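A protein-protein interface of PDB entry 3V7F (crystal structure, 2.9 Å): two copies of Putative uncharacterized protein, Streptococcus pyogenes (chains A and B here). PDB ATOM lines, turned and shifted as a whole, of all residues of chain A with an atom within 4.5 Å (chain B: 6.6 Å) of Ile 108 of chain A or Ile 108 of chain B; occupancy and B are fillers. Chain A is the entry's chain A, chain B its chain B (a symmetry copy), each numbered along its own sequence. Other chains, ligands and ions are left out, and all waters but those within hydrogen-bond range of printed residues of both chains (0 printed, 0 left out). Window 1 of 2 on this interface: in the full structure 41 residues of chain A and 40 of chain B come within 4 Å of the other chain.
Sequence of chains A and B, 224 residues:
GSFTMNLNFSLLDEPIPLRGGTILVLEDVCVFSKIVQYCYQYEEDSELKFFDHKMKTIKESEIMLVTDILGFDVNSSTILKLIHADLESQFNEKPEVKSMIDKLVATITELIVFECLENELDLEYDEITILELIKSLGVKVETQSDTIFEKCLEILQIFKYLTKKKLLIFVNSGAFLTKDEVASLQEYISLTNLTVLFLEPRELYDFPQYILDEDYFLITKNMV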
ATOM      1  N   LEU A 104      32.531 -14.744 -24.124  1.00  0.00           N
ATOM      2  CA  LEU A 104      31.218 -14.210 -23.774  1.00  0.00           C
ATOM      3  C   LEU A 104      30.233 -14.292 -24.940  1.00  0.00           C
ATOM      4  O   LEU A 104      29.069 -14.620 -24.711  1.00  0.00           O
ATOM      5  CB  LEU A 104      31.283 -12.776 -23.222  1.00  0.00           C
ATOM      6  CG  LEU A 104      32.075 -12.565 -21.935  1.00  0.00           C
ATOM      7  CD1 LEU A 104      32.059 -11.115 -21.556  1.00  0.00           C
ATOM      8  CD2 LEU A 104      31.538 -13.439 -20.827  1.00  0.00           C
ATOM      9  N   VAL A 105      30.694 -14.005 -26.163  1.00  0.00           N
ATOM     10  CA  VAL A 105      29.810 -13.986 -27.334  1.00  0.00           C
ATOM     11  C   VAL A 105      29.291 -15.412 -27.583  1.00  0.00           C
ATOM     12  O   VAL A 105      28.066 -15.633 -27.826  1.00  0.00           O
ATOM     13  CB  VAL A 105      30.501 -13.441 -28.622  1.00  0.00           C
ATOM     14  CG1 VAL A 105      29.576 -13.496 -29.811  1.00  0.00           C
ATOM     15  CG2 VAL A 105      30.962 -12.016 -28.454  1.00  0.00           C
ATOM     16  N   ALA A 106      30.218 -16.375 -27.474  1.00  0.00           N
ATOM     17  CA  ALA A 106      29.864 -17.790 -27.544  1.00  0.00           C
ATOM     18  C   ALA A 106      28.719 -18.137 -26.560  1.00  0.00           C
ATOM     19  O   ALA A 106      27.800 -18.905 -26.897  1.00  0.00           O
ATOM     20  CB  ALA A 106      31.075 -18.664 -27.350  1.00  0.00           C
ATOM     21  N   THR A 107      28.726 -17.532 -25.380  1.00  0.00           N
ATOM     22  CA  THR A 107      27.685 -17.879 -24.406  1.00  0.00           C
ATOM     23  C   THR A 107      26.308 -17.347 -24.839  1.00  0.00           C
ATOM     24  O   THR A 107      25.290 -18.072 -24.784  1.00  0.00           O
ATOM     25  CB  THR A 107      28.080 -17.431 -22.966  1.00  0.00           C
ATOM     26  OG1 THR A 107      29.437 -17.791 -22.732  1.00  0.00           O
ATOM     27  CG2 THR A 107      27.251 -18.103 -21.911  1.00  0.00           C
ATOM     28  N   ILE A 108      26.293 -16.084 -25.277  1.00  0.00           N
ATOM     29  CA  ILE A 108      25.094 -15.491 -25.840  1.00  0.00           C
ATOM     30  C   ILE A 108      24.631 -16.354 -27.002  1.00  0.00           C
ATOM     31  O   ILE A 108      23.465 -16.759 -27.043  1.00  0.00           O
ATOM     32  CB  ILE A 108      25.359 -14.103 -26.379  1.00  0.00           C
ATOM     33  CG1 ILE A 108      26.007 -13.216 -25.315  1.00  0.00           C
ATOM     34  CG2 ILE A 108      24.050 -13.490 -26.813  1.00  0.00           C
ATOM     35  CD1 ILE A 108      25.898 -11.683 -25.540  1.00  0.00           C
ATOM     36  N   THR A 109      25.561 -16.668 -27.921  1.00  0.00           N
ATOM     37  CA  THR A 109      25.244 -17.545 -29.056  1.00  0.00           C
ATOM     38  C   THR A 109      24.536 -18.824 -28.624  1.00  0.00           C
ATOM     39  O   THR A 109      23.444 -19.137 -29.112  1.00  0.00           O
ATOM     40  CB  THR A 109      26.449 -17.922 -29.894  1.00  0.00           C
ATOM     41  OG1 THR A 109      27.078 -16.739 -30.406  1.00  0.00           O
ATOM     42  CG2 THR A 109      26.009 -18.844 -31.050  1.00  0.00           C
ATOM     43  N   GLU A 110      25.153 -19.550 -27.699  1.00  0.00           N
ATOM     44  CA  GLU A 110      24.574 -20.746 -27.164  1.00  0.00           C
ATOM     45  C   GLU A 110      23.185 -20.506 -26.591  1.00  0.00           C
ATOM     46  O   GLU A 110      22.275 -21.285 -26.859  1.00  0.00           O
ATOM     47  CB  GLU A 110      25.500 -21.303 -26.109  1.00  0.00           C
ATOM     48  CG  GLU A 110      25.004 -22.568 -25.452  1.00  0.00           C
ATOM     49  CD  GLU A 110      25.870 -22.970 -24.267  1.00  0.00           C
ATOM     50  OE1 GLU A 110      26.778 -22.169 -23.891  1.00  0.00           O
ATOM     51  OE2 GLU A 110      25.636 -24.086 -23.722  1.00  0.00           O
ATOM     52  N   LEU A 111      22.994 -19.438 -25.830  1.00  0.00           N
ATOM     53  CA  LEU A 111      21.675 -19.235 -25.221  1.00  0.00           C
ATOM     54  C   LEU A 111      20.661 -18.941 -26.294  1.00  0.00           C
ATOM     55  O   LEU A 111      19.477 -19.298 -26.143  1.00  0.00           O
ATOM     56  CB  LEU A 111      21.660 -18.116 -24.196  1.00  0.00           C
ATOM     57  CG  LEU A 111      22.685 -18.159 -23.070  1.00  0.00           C
ATOM     58  CD1 LEU A 111      22.716 -16.811 -22.380  1.00  0.00           C
ATOM     59  CD2 LEU A 111      22.297 -19.225 -22.135  1.00  0.00           C
ATOM     60  N   ILE A 112      21.123 -18.305 -27.378  1.00  0.00           N
ATOM     61  CA  ILE A 112      20.264 -18.079 -28.546  1.00  0.00           C
ATOM     62  C   ILE A 112      19.964 -19.374 -29.360  1.00  0.00           C
ATOM     63  O   ILE A 112      18.793 -19.717 -29.590  1.00  0.00           O
ATOM     64  CB  ILE A 112      20.781 -16.955 -29.466  1.00  0.00           C
ATOM     65  CG1 ILE A 112      20.990 -15.689 -28.642  1.00  0.00           C
ATOM     66  CG2 ILE A 112      19.768 -16.735 -30.609  1.00  0.00           C
ATOM     67  CD1 ILE A 112      21.466 -14.532 -29.403  1.00  0.00           C
ATOM     68  N   LEU A 133      28.735  -6.188 -33.094  1.00  0.00           N
ATOM     69  CA  LEU A 133      28.365  -5.720 -31.762  1.00  0.00           C
ATOM     70  C   LEU A 133      28.593  -4.219 -31.687  1.00  0.00           C
ATOM     71  O   LEU A 133      27.730  -3.453 -31.167  1.00  0.00           O
ATOM     72  CB  LEU A 133      29.164  -6.441 -30.713  1.00  0.00           C
ATOM     73  CG  LEU A 133      28.761  -7.903 -30.604  1.00  0.00           C
ATOM     74  CD1 LEU A 133      29.838  -8.610 -29.851  1.00  0.00           C
ATOM     75  CD2 LEU A 133      27.453  -8.079 -29.863  1.00  0.00           C
ATOM     76  N   PHE B  91      12.896 -15.460 -24.669  1.00  0.00           N
ATOM     77  CA  PHE B  91      13.702 -14.888 -23.612  1.00  0.00           C
ATOM     78  C   PHE B  91      12.823 -14.255 -22.555  1.00  0.00           C
ATOM     79  O   PHE B  91      12.800 -14.733 -21.437  1.00  0.00           O
ATOM     80  CB  PHE B  91      14.751 -13.918 -24.172  1.00  0.00           C
ATOM     81  CG  PHE B  91      15.932 -14.606 -24.823  1.00  0.00           C
ATOM     82  CD1 PHE B  91      16.844 -15.329 -24.074  1.00  0.00           C
ATOM     83  CD2 PHE B  91      16.143 -14.521 -26.167  1.00  0.00           C
ATOM     84  CE1 PHE B  91      17.936 -15.957 -24.674  1.00  0.00           C
ATOM     85  CE2 PHE B  91      17.243 -15.142 -26.756  1.00  0.00           C
ATOM     86  CZ  PHE B  91      18.134 -15.859 -26.013  1.00  0.00           C
ATOM     87  N   MET B 100      20.771 -13.553 -17.642  1.00  0.00           N
ATOM     88  CA  MET B 100      22.097 -13.980 -18.067  1.00  0.00           C
ATOM     89  C   MET B 100      22.508 -13.275 -19.365  1.00  0.00           C
ATOM     90  O   MET B 100      23.659 -12.873 -19.527  1.00  0.00           O
ATOM     91  CB  MET B 100      22.163 -15.512 -18.206  1.00  0.00           C
ATOM     92  CG  MET B 100      23.570 -16.092 -18.377  1.00  0.00           C
ATOM     93  SD  MET B 100      24.688 -15.651 -16.977  1.00  0.00           S
ATOM     94  CE  MET B 100      26.100 -16.788 -17.172  1.00  0.00           C
ATOM     95  N   ILE B 101      21.566 -13.124 -20.288  1.00  0.00           N
ATOM     96  CA  ILE B 101      21.803 -12.386 -21.517  1.00  0.00           C
ATOM     97  C   ILE B 101      22.208 -10.993 -21.108  1.00  0.00           C
ATOM     98  O   ILE B 101      23.262 -10.526 -21.504  1.00  0.00           O
ATOM     99  CB  ILE B 101      20.549 -12.372 -22.426  1.00  0.00           C
ATOM    100  CG1 ILE B 101      20.553 -13.584 -23.323  1.00  0.00           C
ATOM    101  CG2 ILE B 101      20.515 -11.176 -23.304  1.00  0.00           C
ATOM    102  CD1 ILE B 101      21.583 -13.510 -24.356  1.00  0.00           C
ATOM    103  N   LYS B 103      23.436  -9.606 -18.273  1.00  0.00           N
ATOM    104  CA  LYS B 103      24.763  -9.574 -17.703  1.00  0.00           C
ATOM    105  C   LYS B 103      25.831  -9.692 -18.773  1.00  0.00           C
ATOM    106  O   LYS B 103      26.808  -8.933 -18.769  1.00  0.00           O
ATOM    107  CB  LYS B 103      24.921 -10.671 -16.642  1.00  0.00           C
ATOM    108  CG  LYS B 103      24.113 -10.353 -15.389  1.00  0.00           C
ATOM    109  CD  LYS B 103      24.041 -11.476 -14.343  1.00  0.00           C
ATOM    110  CE  LYS B 103      22.897 -11.079 -13.368  1.00  0.00           C
ATOM    111  NZ  LYS B 103      22.522 -12.061 -12.288  1.00  0.00           N
ATOM    112  N   LEU B 104      25.647 -10.623 -19.697  1.00  0.00           N
ATOM    113  CA  LEU B 104      26.611 -10.772 -20.750  1.00  0.00           C
ATOM    114  C   LEU B 104      26.685  -9.515 -21.628  1.00  0.00           C
ATOM    115  O   LEU B 104      27.779  -9.011 -21.902  1.00  0.00           O
ATOM    116  CB  LEU B 104      26.301 -12.005 -21.571  1.00  0.00           C
ATOM    117  CG  LEU B 104      26.643 -13.359 -20.944  1.00  0.00           C
ATOM    118  CD1 LEU B 104      26.046 -14.451 -21.727  1.00  0.00           C
ATOM    119  CD2 LEU B 104      28.123 -13.586 -20.876  1.00  0.00           C
ATOM    120  N   VAL B 105      25.554  -8.960 -22.050  1.00  0.00           N
ATOM    121  CA  VAL B 105      25.656  -7.771 -22.891  1.00  0.00           C
ATOM    122  C   VAL B 105      26.254  -6.590 -22.116  1.00  0.00           C
ATOM    123  O   VAL B 105      27.202  -5.933 -22.583  1.00  0.00           O
ATOM    124  CB  VAL B 105      24.320  -7.371 -23.509  1.00  0.00           C
ATOM    125  CG1 VAL B 105      24.442  -6.037 -24.250  1.00  0.00           C
ATOM    126  CG2 VAL B 105      23.851  -8.459 -24.433  1.00  0.00           C
ATOM    127  N   ALA B 106      25.713  -6.323 -20.932  1.00  0.00           N
ATOM    128  CA  ALA B 106      26.221  -5.233 -20.114  1.00  0.00           C
ATOM    129  C   ALA B 106      27.741  -5.291 -20.019  1.00  0.00           C
ATOM    130  O   ALA B 106      28.399  -4.271 -20.142  1.00  0.00           O
ATOM    131  CB  ALA B 106      25.578  -5.245 -18.738  1.00  0.00           C
ATOM    132  N   THR B 107      28.286  -6.488 -19.847  1.00  0.00           N
ATOM    133  CA  THR B 107      29.732  -6.660 -19.732  1.00  0.00           C
ATOM    134  C   THR B 107      30.423  -6.385 -21.051  1.00  0.00           C
ATOM    135  O   THR B 107      31.346  -5.555 -21.112  1.00  0.00           O
ATOM    136  CB  THR B 107      30.141  -8.096 -19.258  1.00  0.00           C
ATOM    137  OG1 THR B 107      29.709  -8.316 -17.911  1.00  0.00           O
ATOM    138  CG2 THR B 107      31.633  -8.295 -19.297  1.00  0.00           C
ATOM    139  N   ILE B 108      29.988  -7.093 -22.098  1.00  0.00           N
ATOM    140  CA  ILE B 108      30.494  -6.864 -23.464  1.00  0.00           C
ATOM    141  C   ILE B 108      30.442  -5.388 -23.930  1.00  0.00           C
ATOM    142  O   ILE B 108      31.385  -4.890 -24.553  1.00  0.00           O
ATOM    143  CB  ILE B 108      29.747  -7.697 -24.475  1.00  0.00           C
ATOM    144  CG1 ILE B 108      30.176  -9.171 -24.360  1.00  0.00           C
ATOM    145  CG2 ILE B 108      30.082  -7.170 -25.835  1.00  0.00           C
ATOM    146  CD1 ILE B 108      29.539 -10.092 -25.376  1.00  0.00           C
ATOM    147  N   THR B 109      29.355  -4.695 -23.597  1.00  0.00           N
ATOM    148  CA  THR B 109      29.278  -3.290 -23.826  1.00  0.00           C
ATOM    149  C   THR B 109      30.383  -2.509 -23.140  1.00  0.00           C
ATOM    150  O   THR B 109      31.056  -1.695 -23.791  1.00  0.00           O
ATOM    151  CB  THR B 109      28.024  -2.783 -23.325  1.00  0.00           C
ATOM    152  OG1 THR B 109      26.977  -3.473 -24.010  1.00  0.00           O
ATOM    153  CG2 THR B 109      27.950  -1.315 -23.610  1.00  0.00           C
ATOM    154  N   GLU B 110      30.593  -2.735 -21.850  1.00  0.00           N
ATOM    155  CA  GLU B 110      31.647  -2.022 -21.201  1.00  0.00           C
ATOM    156  C   GLU B 110      32.956  -2.252 -21.879  1.00  0.00           C
ATOM    157  O   GLU B 110      33.713  -1.317 -22.098  1.00  0.00           O
ATOM    158  CB  GLU B 110      31.758  -2.387 -19.746  1.00  0.00           C
ATOM    159  CG  GLU B 110      31.212  -1.286 -18.912  1.00  0.00           C
ATOM    160  CD  GLU B 110      31.389  -1.515 -17.455  1.00  0.00           C
ATOM    161  OE1 GLU B 110      30.353  -1.378 -16.764  1.00  0.00           O
ATOM    162  OE2 GLU B 110      32.539  -1.814 -17.002  1.00  0.00           O
ATOM    163  N   LEU B 111      33.237  -3.485 -22.247  1.00  0.00           N
ATOM    164  CA  LEU B 111      34.536  -3.748 -22.820  1.00  0.00           C
ATOM    165  C   LEU B 111      34.790  -2.978 -24.123  1.00  0.00           C
ATOM    166  O   LEU B 111      35.939  -2.617 -24.440  1.00  0.00           O
ATOM    167  CB  LEU B 111      34.763  -5.241 -22.948  1.00  0.00           C
ATOM    168  CG  LEU B 111      34.778  -5.961 -21.576  1.00  0.00           C
ATOM    169  CD1 LEU B 111      34.837  -7.479 -21.759  1.00  0.00           C
ATOM    170  CD2 LEU B 111      35.912  -5.518 -20.702  1.00  0.00           C
ATOM    171  N   ILE B 112      33.713  -2.689 -24.847  1.00  0.00           N
ATOM    172  CA  ILE B 112      33.810  -1.921 -26.084  1.00  0.00           C
ATOM    173  C   ILE B 112      33.940  -0.428 -25.762  1.00  0.00           C
ATOM    174  O   ILE B 112      34.864   0.272 -26.241  1.00  0.00           O
ATOM    175  CB  ILE B 112      32.597  -2.170 -27.004  1.00  0.00           C
ATOM    176  CG1 ILE B 112      32.522  -3.643 -27.419  1.00  0.00           C
ATOM    177  CG2 ILE B 112      32.682  -1.294 -28.277  1.00  0.00           C
ATOM    178  CD1 ILE B 112      31.172  -4.049 -27.984  1.00  0.00           C
ATOM    179  N   VAL B 113      33.004   0.062 -24.948  1.00  0.00           N
ATOM    180  CA  VAL B 113      33.077   1.425 -24.467  1.00  0.00           C
ATOM    181  C   VAL B 113      34.477   1.650 -23.907  1.00  0.00           C
ATOM    182  O   VAL B 113      34.998   2.769 -23.962  1.00  0.00           O
ATOM    183  CB  VAL B 113      32.015   1.706 -23.392  1.00  0.00           C
ATOM    184  CG1 VAL B 113      32.263   3.053 -22.720  1.00  0.00           C
ATOM    185  CG2 VAL B 113      30.644   1.680 -24.014  1.00  0.00           C
ATOM    186  N   ILE B 128      22.937  -2.434 -26.813  1.00  0.00           N
ATOM    187  CA  ILE B 128      22.831  -3.623 -27.679  1.00  0.00           C
ATOM    188  C   ILE B 128      21.648  -4.435 -27.193  1.00  0.00           C
ATOM    189  O   ILE B 128      21.550  -4.727 -26.006  1.00  0.00           O
ATOM    190  CB  ILE B 128      24.088  -4.502 -27.655  1.00  0.00           C
ATOM    191  CG1 ILE B 128      25.329  -3.687 -27.979  1.00  0.00           C
ATOM    192  CG2 ILE B 128      23.965  -5.649 -28.617  1.00  0.00           C
ATOM    193  CD1 ILE B 128      26.587  -4.523 -28.053  1.00  0.00           C
ATOM    194  N   LEU B 133      21.223  -8.952 -31.422  1.00  0.00           N
ATOM    195  CA  LEU B 133      21.995 -10.178 -31.274  1.00  0.00           C
ATOM    196  C   LEU B 133      21.437 -11.273 -32.151  1.00  0.00           C
ATOM    197  O   LEU B 133      22.165 -11.916 -32.900  1.00  0.00           O
ATOM    198  CB  LEU B 133      21.975 -10.620 -29.843  1.00  0.00           C
ATOM    199  CG  LEU B 133      22.736  -9.644 -28.968  1.00  0.00           C
ATOM    200  CD1 LEU B 133      22.669 -10.056 -27.516  1.00  0.00           C
ATOM    201  CD2 LEU B 133      24.143  -9.614 -29.439  1.00  0.00           C
ATOM    202  N   LEU B 137      23.249 -12.688 -35.463  1.00  0.00           N
ATOM    203  CA  LEU B 137      23.596 -14.070 -35.532  1.00  0.00           C
ATOM    204  C   LEU B 137      23.102 -14.660 -36.841  1.00  0.00           C
ATOM    205  O   LEU B 137      23.646 -15.636 -37.316  1.00  0.00           O
ATOM    206  CB  LEU B 137      23.017 -14.803 -34.356  1.00  0.00           C
ATOM    207  CG  LEU B 137      23.284 -16.310 -34.305  1.00  0.00           C
ATOM    208  CD1 LEU B 137      24.780 -16.703 -34.251  1.00  0.00           C
ATOM    209  CD2 LEU B 137      22.565 -16.850 -33.121  1.00  0.00           C
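Among the printed residues, pairs that only touch across the chains: Leu 104 of chain A with Leu 104 of chain B (3.4 Å), Leu 104 of chain A with Thr 107 of chain B (3.6 Å), Leu 104 of chain A with Ile 108 of chain B (3.9 Å), Val 105 of chain A with Ile 108 of chain B (3.9 Å), Thr 107 of chain A with Leu 104 of chain B (3.8 Å), Ile 108 of chain A with Ile 101 of chain B (3.5 Å), Ile 108 of chain A with Leu 104 of chain B (3.8 Å), Ile 108 of chain A with Val 105 of chain B (3.98 Å), Ile 108 of chain A with Ile 108 of chain B (3.98 Å), Ile 108 of chain A with Leu 133 of chain B (3.8 Å), Leu 111 of chain A with Phe 91 of chain B (3.7 Å), Leu 111 of chain A with Ile 101 of chain B (3.998 Å), Ile 112 of chain A with Phe 91 of chain B (3.9 Å), Ile 112 of chain A with Leu 133 of chain B (3.97 Å), Ile 112 of chain A with Leu 137 of chain B (3.8 Å), Leu 133 of chain A with Ile 128 of chain B (3.5 Å) and Leu 133 of chain A with Leu 133 of chain B (3.7 Å).
Of chain B, only Ile 101 (3.5 Å), Leu 104 (3.8 Å), Val 105 (3.98 Å), Ile 108 (3.98 Å) and Leu 133 (3.8 Å) come within 4 Å of Ile 108 of chain A. Ile 108 of chain B touches just these residues of chain A: Leu 104, Val 105 and Ile 108. Printed residues of chain A within 4 Å of Ile 128 of chain B: Leu 133. Of the printed residues of chain B, Ile 112 of chain A touches Phe 91, Leu 133 and Leu 137. Printed residues of chain A within 4 Å of Ile 101 of chain B: Ile 108 (3.5 Å) and Leu 111 (3.998 Å). Printed residues of chain B within 4 Å of Leu 111 of chain A: Phe 91 (3.7 Å) and Ile 101 (3.998 Å). Of the printed residues of chain A, Phe 91 of chain B touches Leu 111 (3.7 Å) and Ile 112 (3.9 Å). The nearest residue of chain B that does not touch Ile 108 of chain A is Phe 91 of chain B (5.5 Å). The nearest residue of chain A that does not touch Ile 108 of chain B is Leu 133 of chain A (4.3 Å).
Along chain B the printed residues that touch a printed residue of chain A span positions 91 to 137. Of the 10 printed residues of chain A, 7 touch a printed residue of chain B. Printed residues of chain A that touch a printed residue of chain B: Leu 104, Val 105, Thr 107, Ile 108, Leu 111, Ile 112 and Leu 133. Hydrophobic or aromatic side chains of chain A within 4 Å of the printed part of chain B: Leu 104, Val 105, Ile 108, Leu 111, Ile 112 and Leu 133. Among the printed residues, no Asp or Glu carboxylate lies within 4 Å of a Lys or Arg side-chain nitrogen of the other chain.
Leu 104 of chain A touches its own counterpart, Leu 104 of chain B. Leu 104 of chain A touches Ile 108 of chain B, and with the chains exchanged Ile 108 of chain A touches Leu 104 of chain B. Ile 108 of chain A touches Leu 133 of chain B, but with the chains exchanged Leu 133 of chain A does not touch Ile 108 of chain B (4.3 Å). Leu 133 of chain A touches its own counterpart, Leu 133 of chain B. Positions printed for both chains: 104, 105, 106, 107, 108, 109, 110, 111, 112 and 133.
OG1 of Thr 107 of chain B lies within hydrogen-bond range of O of Lys 103 of chain B, 3.1 Å away. The backbone carbonyl oxygen (O) of Val 105 of chain B is in hydrogen-bond range of the side-chain hydroxyl (OG1) of Thr 109 of chain B (2.9 Å). The side-chain hydroxyl (OG1) of Thr 109 of chain A lies within hydrogen-bond range of the backbone carbonyl oxygen (O) of Val 105 of chain A (3.0 Å).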
